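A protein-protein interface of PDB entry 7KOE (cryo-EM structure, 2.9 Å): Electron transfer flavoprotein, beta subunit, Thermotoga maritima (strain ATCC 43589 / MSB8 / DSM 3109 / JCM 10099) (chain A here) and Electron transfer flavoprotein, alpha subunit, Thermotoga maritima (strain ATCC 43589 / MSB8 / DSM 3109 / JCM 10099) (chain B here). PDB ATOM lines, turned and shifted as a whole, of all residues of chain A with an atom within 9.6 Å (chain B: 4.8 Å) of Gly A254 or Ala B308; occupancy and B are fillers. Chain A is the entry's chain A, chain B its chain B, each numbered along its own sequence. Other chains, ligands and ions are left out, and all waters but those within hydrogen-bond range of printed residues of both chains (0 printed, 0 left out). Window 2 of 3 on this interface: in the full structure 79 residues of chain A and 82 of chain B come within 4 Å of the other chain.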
ATOM      1  N   ALA A 250       1.919   3.824 -13.756  1.00  0.00           N
ATOM      2  CA  ALA A 250       1.433   2.544 -13.189  1.00  0.00           C
ATOM      3  C   ALA A 250       0.017   2.256 -13.703  1.00  0.00           C
ATOM      4  O   ALA A 250      -0.887   2.062 -12.867  1.00  0.00           O
ATOM      5  CB  ALA A 250       1.473   2.600 -11.682  1.00  0.00           C
ATOM      6  N   ARG A 251      -0.154   2.233 -15.030  1.00  0.00           N
ATOM      7  CA  ARG A 251      -1.476   1.964 -15.660  1.00  0.00           C
ATOM      8  C   ARG A 251      -2.535   2.876 -15.031  1.00  0.00           C
ATOM      9  O   ARG A 251      -2.301   4.100 -14.971  1.00  0.00           O
ATOM     10  CB  ARG A 251      -1.853   0.487 -15.504  1.00  0.00           C
ATOM     11  CG  ARG A 251      -1.904  -0.283 -16.816  1.00  0.00           C
ATOM     12  CD  ARG A 251      -3.210  -1.035 -16.993  1.00  0.00           C
ATOM     13  NE  ARG A 251      -3.874  -0.705 -18.246  1.00  0.00           N
ATOM     14  CZ  ARG A 251      -3.276  -0.682 -19.431  1.00  0.00           C
ATOM     15  NH1 ARG A 251      -1.990  -0.972 -19.529  1.00  0.00           N
ATOM     16  NH2 ARG A 251      -3.965  -0.370 -20.514  1.00  0.00           N
ATOM     17  N   LYS A 252      -3.651   2.294 -14.583  1.00  0.00           N
ATOM     18  CA  LYS A 252      -4.752   3.070 -13.952  1.00  0.00           C
ATOM     19  C   LYS A 252      -5.686   2.108 -13.209  1.00  0.00           C
ATOM     20  O   LYS A 252      -6.265   1.220 -13.866  1.00  0.00           O
ATOM     21  CB  LYS A 252      -5.517   3.869 -15.014  1.00  0.00           C
ATOM     22  CG  LYS A 252      -5.763   5.333 -14.675  1.00  0.00           C
ATOM     23  CD  LYS A 252      -5.712   6.245 -15.884  1.00  0.00           C
ATOM     24  CE  LYS A 252      -5.457   5.501 -17.176  1.00  0.00           C
ATOM     25  NZ  LYS A 252      -4.105   4.895 -17.203  1.00  0.00           N
ATOM     26  N   GLY A 253      -5.819   2.286 -11.890  1.00  0.00           N
ATOM     27  CA  GLY A 253      -6.688   1.423 -11.067  1.00  0.00           C
ATOM     28  C   GLY A 253      -8.098   1.344 -11.629  1.00  0.00           C
ATOM     29  O   GLY A 253      -8.695   2.409 -11.875  1.00  0.00           O
ATOM     30  N   GLY A 254      -8.608   0.123 -11.823  1.00  0.00           N
ATOM     31  CA  GLY A 254      -9.966  -0.082 -12.362  1.00  0.00           C
ATOM     32  C   GLY A 254     -10.992  -0.247 -11.254  1.00  0.00           C
ATOM     33  O   GLY A 254     -10.693   0.150 -10.110  1.00  0.00           O
ATOM     34  N   ASP A 255     -12.158  -0.811 -11.583  1.00  0.00           N
ATOM     35  CA  ASP A 255     -13.240  -1.026 -10.584  1.00  0.00           C
ATOM     36  C   ASP A 255     -14.132  -2.185 -11.046  1.00  0.00           C
ATOM     37  O   ASP A 255     -14.511  -2.202 -12.235  1.00  0.00           O
ATOM     38  CB  ASP A 255     -14.047   0.254 -10.354  1.00  0.00           C
ATOM     39  CG  ASP A 255     -14.249   0.583  -8.885  1.00  0.00           C
ATOM     40  OD1 ASP A 255     -13.907  -0.270  -8.042  1.00  0.00           O
ATOM     41  OD2 ASP A 255     -14.743   1.691  -8.596  1.00  0.00           O
ATOM     42  N   ILE A 256     -14.447  -3.111 -10.135  1.00  0.00           N
ATOM     43  CA  ILE A 256     -15.308  -4.287 -10.463  1.00  0.00           C
ATOM     44  C   ILE A 256     -16.648  -3.779 -11.010  1.00  0.00           C
ATOM     45  O   ILE A 256     -17.558  -3.520 -10.198  1.00  0.00           O
ATOM     46  CB  ILE A 256     -15.500  -5.188  -9.227  1.00  0.00           C
ATOM     47  CG1 ILE A 256     -14.326  -5.070  -8.250  1.00  0.00           C
ATOM     48  CG2 ILE A 256     -15.745  -6.631  -9.642  1.00  0.00           C
ATOM     49  CD1 ILE A 256     -12.979  -5.356  -8.874  1.00  0.00           C
ATOM     50  N   ILE A 257     -16.752  -3.646 -12.337  1.00  0.00           N
ATOM     51  CA  ILE A 257     -18.005  -3.159 -12.990  1.00  0.00           C
ATOM     52  C   ILE A 257     -19.180  -4.016 -12.505  1.00  0.00           C
ATOM     53  O   ILE A 257     -20.185  -3.436 -12.048  1.00  0.00           O
ATOM     54  CB  ILE A 257     -17.869  -3.191 -14.526  1.00  0.00           C
ATOM     55  CG1 ILE A 257     -17.115  -1.968 -15.054  1.00  0.00           C
ATOM     56  CG2 ILE A 257     -19.232  -3.341 -15.184  1.00  0.00           C
ATOM     57  CD1 ILE A 257     -16.950  -0.862 -14.038  1.00  0.00           C
ATOM     58  N   PHE A 277     -14.983   4.676 -22.642  1.00  0.00           N
ATOM     59  CA  PHE A 277     -13.584   4.733 -23.038  1.00  0.00           C
ATOM     60  C   PHE A 277     -13.454   5.232 -24.470  1.00  0.00           C
ATOM     61  O   PHE A 277     -14.330   5.015 -25.309  1.00  0.00           O
ATOM     62  CB  PHE A 277     -12.918   3.360 -22.905  1.00  0.00           C
ATOM     63  CG  PHE A 277     -12.739   2.910 -21.484  1.00  0.00           C
ATOM     64  CD1 PHE A 277     -11.780   3.492 -20.674  1.00  0.00           C
ATOM     65  CD2 PHE A 277     -13.533   1.904 -20.960  1.00  0.00           C
ATOM     66  CE1 PHE A 277     -11.618   3.079 -19.364  1.00  0.00           C
ATOM     67  CE2 PHE A 277     -13.377   1.489 -19.652  1.00  0.00           C
ATOM     68  CZ  PHE A 277     -12.418   2.077 -18.854  1.00  0.00           C
ATOM     69  N   ILE B 293      -8.226  -3.185 -20.502  1.00  0.00           N
ATOM     70  CA  ILE B 293      -8.053  -4.529 -19.969  1.00  0.00           C
ATOM     71  C   ILE B 293      -9.321  -4.882 -19.210  1.00  0.00           C
ATOM     72  O   ILE B 293      -9.648  -4.242 -18.205  1.00  0.00           O
ATOM     73  CB  ILE B 293      -6.820  -4.644 -19.064  1.00  0.00           C
ATOM     74  CG1 ILE B 293      -5.546  -4.433 -19.875  1.00  0.00           C
ATOM     75  CG2 ILE B 293      -6.784  -5.995 -18.376  1.00  0.00           C
ATOM     76  CD1 ILE B 293      -4.302  -4.402 -19.044  1.00  0.00           C
ATOM     77  N   ALA B 295     -11.206  -7.818 -17.053  1.00  0.00           N
ATOM     78  CA  ALA B 295     -10.860  -8.986 -16.256  1.00  0.00           C
ATOM     79  C   ALA B 295     -12.131  -9.644 -15.746  1.00  0.00           C
ATOM     80  O   ALA B 295     -12.907  -9.020 -15.018  1.00  0.00           O
ATOM     81  CB  ALA B 295      -9.956  -8.603 -15.087  1.00  0.00           C
ATOM     82  N   ILE B 304      -5.058  -9.383 -11.209  1.00  0.00           N
ATOM     83  CA  ILE B 304      -5.417  -8.815 -12.501  1.00  0.00           C
ATOM     84  C   ILE B 304      -6.237  -7.544 -12.318  1.00  0.00           C
ATOM     85  O   ILE B 304      -6.189  -6.646 -13.166  1.00  0.00           O
ATOM     86  CB  ILE B 304      -6.140  -9.879 -13.359  1.00  0.00           C
ATOM     87  CG1 ILE B 304      -6.330  -9.412 -14.804  1.00  0.00           C
ATOM     88  CG2 ILE B 304      -7.457 -10.310 -12.731  1.00  0.00           C
ATOM     89  CD1 ILE B 304      -5.054  -9.284 -15.578  1.00  0.00           C
ATOM     90  N   PHE B 305      -6.933  -7.409 -11.189  1.00  0.00           N
ATOM     91  CA  PHE B 305      -7.753  -6.241 -10.905  1.00  0.00           C
ATOM     92  C   PHE B 305      -6.931  -5.004 -10.572  1.00  0.00           C
ATOM     93  O   PHE B 305      -7.481  -3.898 -10.570  1.00  0.00           O
ATOM     94  CB  PHE B 305      -8.712  -6.552  -9.758  1.00  0.00           C
ATOM     95  CG  PHE B 305      -9.787  -7.528 -10.125  1.00  0.00           C
ATOM     96  CD1 PHE B 305     -10.373  -7.494 -11.379  1.00  0.00           C
ATOM     97  CD2 PHE B 305     -10.212  -8.482  -9.219  1.00  0.00           C
ATOM     98  CE1 PHE B 305     -11.362  -8.391 -11.720  1.00  0.00           C
ATOM     99  CE2 PHE B 305     -11.202  -9.379  -9.557  1.00  0.00           C
ATOM    100  CZ  PHE B 305     -11.777  -9.331 -10.807  1.00  0.00           C
ATOM    101  N   ASP B 306      -5.640  -5.156 -10.294  1.00  0.00           N
ATOM    102  CA  ASP B 306      -4.755  -4.017 -10.115  1.00  0.00           C
ATOM    103  C   ASP B 306      -4.255  -3.450 -11.437  1.00  0.00           C
ATOM    104  O   ASP B 306      -3.640  -2.380 -11.443  1.00  0.00           O
ATOM    105  CB  ASP B 306      -3.564  -4.410  -9.239  1.00  0.00           C
ATOM    106  CG  ASP B 306      -3.968  -4.707  -7.811  1.00  0.00           C
ATOM    107  OD1 ASP B 306      -4.966  -4.122  -7.342  1.00  0.00           O
ATOM    108  OD2 ASP B 306      -3.288  -5.525  -7.156  1.00  0.00           O
ATOM    109  N   ILE B 307      -4.500  -4.141 -12.546  1.00  0.00           N
ATOM    110  CA  ILE B 307      -4.168  -3.633 -13.871  1.00  0.00           C
ATOM    111  C   ILE B 307      -5.392  -3.487 -14.762  1.00  0.00           C
ATOM    112  O   ILE B 307      -5.313  -2.803 -15.794  1.00  0.00           O
ATOM    113  CB  ILE B 307      -3.099  -4.514 -14.561  1.00  0.00           C
ATOM    114  CG1 ILE B 307      -2.213  -3.683 -15.492  1.00  0.00           C
ATOM    115  CG2 ILE B 307      -3.723  -5.688 -15.307  1.00  0.00           C
ATOM    116  CD1 ILE B 307      -1.038  -4.441 -16.053  1.00  0.00           C
ATOM    117  N   ALA B 308      -6.527  -4.068 -14.385  1.00  0.00           N
ATOM    118  CA  ALA B 308      -7.701  -4.055 -15.241  1.00  0.00           C
ATOM    119  C   ALA B 308      -8.378  -2.692 -15.230  1.00  0.00           C
ATOM    120  O   ALA B 308      -8.355  -1.967 -14.233  1.00  0.00           O
ATOM    121  CB  ALA B 308      -8.698  -5.120 -14.794  1.00  0.00           C
ATOM    122  N   ASP B 309      -8.991  -2.351 -16.361  1.00  0.00           N
ATOM    123  CA  ASP B 309      -9.828  -1.168 -16.453  1.00  0.00           C
ATOM    124  C   ASP B 309     -11.290  -1.468 -16.170  1.00  0.00           C
ATOM    125  O   ASP B 309     -11.995  -0.606 -15.639  1.00  0.00           O
ATOM    126  CB  ASP B 309      -9.704  -0.536 -17.841  1.00  0.00           C
ATOM    127  CG  ASP B 309      -8.346   0.082 -18.074  1.00  0.00           C
ATOM    128  OD1 ASP B 309      -7.725   0.527 -17.087  1.00  0.00           O
ATOM    129  OD2 ASP B 309      -7.898   0.124 -19.236  1.00  0.00           O
ATOM    130  N   ILE B 310     -11.748  -2.670 -16.505  1.00  0.00           N
ATOM    131  CA  ILE B 310     -13.110  -3.114 -16.246  1.00  0.00           C
ATOM    132  C   ILE B 310     -13.013  -4.458 -15.541  1.00  0.00           C
ATOM    133  O   ILE B 310     -12.452  -5.409 -16.094  1.00  0.00           O
ATOM    134  CB  ILE B 310     -13.928  -3.237 -17.545  1.00  0.00           C
ATOM    135  CG1 ILE B 310     -14.224  -1.858 -18.128  1.00  0.00           C
ATOM    136  CG2 ILE B 310     -15.217  -3.977 -17.307  1.00  0.00           C
ATOM    137  CD1 ILE B 310     -14.799  -1.911 -19.516  1.00  0.00           C
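N of Gly A254 sits close to O of Ala B308 (3.2 Å).
The backbone carbonyl oxygen (O) of Ile B293 sits at hydrogen-bond distance from the backbone NH (N) of Asp B309, at 2.7 Å. N of Ile B310 sits at hydrogen-bond distance from O of Ile B293 (3.1 Å). The backbone carbonyl oxygen of Ile B310 lies within hydrogen-bond range of the backbone NH of Ala B295.
Among the printed residues, merely in contact across the chains: Arg A251 with Ile B307, Ile A257 with Ile B310, Lys A252 with Asp B309, Phe A277 with Ile B310, Arg A251 with Ile B293, Lys A252 with Ala B308, Gly A254 with Asp B309 and Phe A277 with Asp B309.
Gly A254 touches just these residues of chain B: Ala B308 (3.1 Å) and Asp B309 (3.9 Å). Printed residues of chain A within 4 Å of Ala B308: Lys A252 (3.8 Å) and Gly A254 (3.1 Å). Of chain A, only Arg A251 comes within 4 Å of Ile B293. Asp B309 touches just these residues of chain A: Lys A252, Gly A254 and Phe A277. Printed residues of chain B within 4 Å of Lys A252: Ala B308 and Asp B309. Printed residues of chain B within 4 Å of Arg A251: Ile B293 (3.8 Å) and Ile B307 (3.0 Å). Of the printed residues of chain A, Ile B307 touches Arg A251 (3.0 Å). Of the printed residues of chain B, Ile A257 touches Ile B310 (3.6 Å). Ala B295 touches none of the printed residues of chain A.
Of the 9 printed residues of chain A, 5 touch a printed residue of chain B. Printed residues of chain A that touch a printed residue of chain B: Arg A251, Lys A252, Gly A254, Ile A257 and Phe A277. Printed residues of chain B that touch a printed residue of chain A: Ile B293, Ile B307, Ala B308, Asp B309 and Ile B310. Hydrophobic or aromatic side chains of chain B within 4 Å of the printed part of chain A: Ile B293, Ile B307 and Ile B310.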
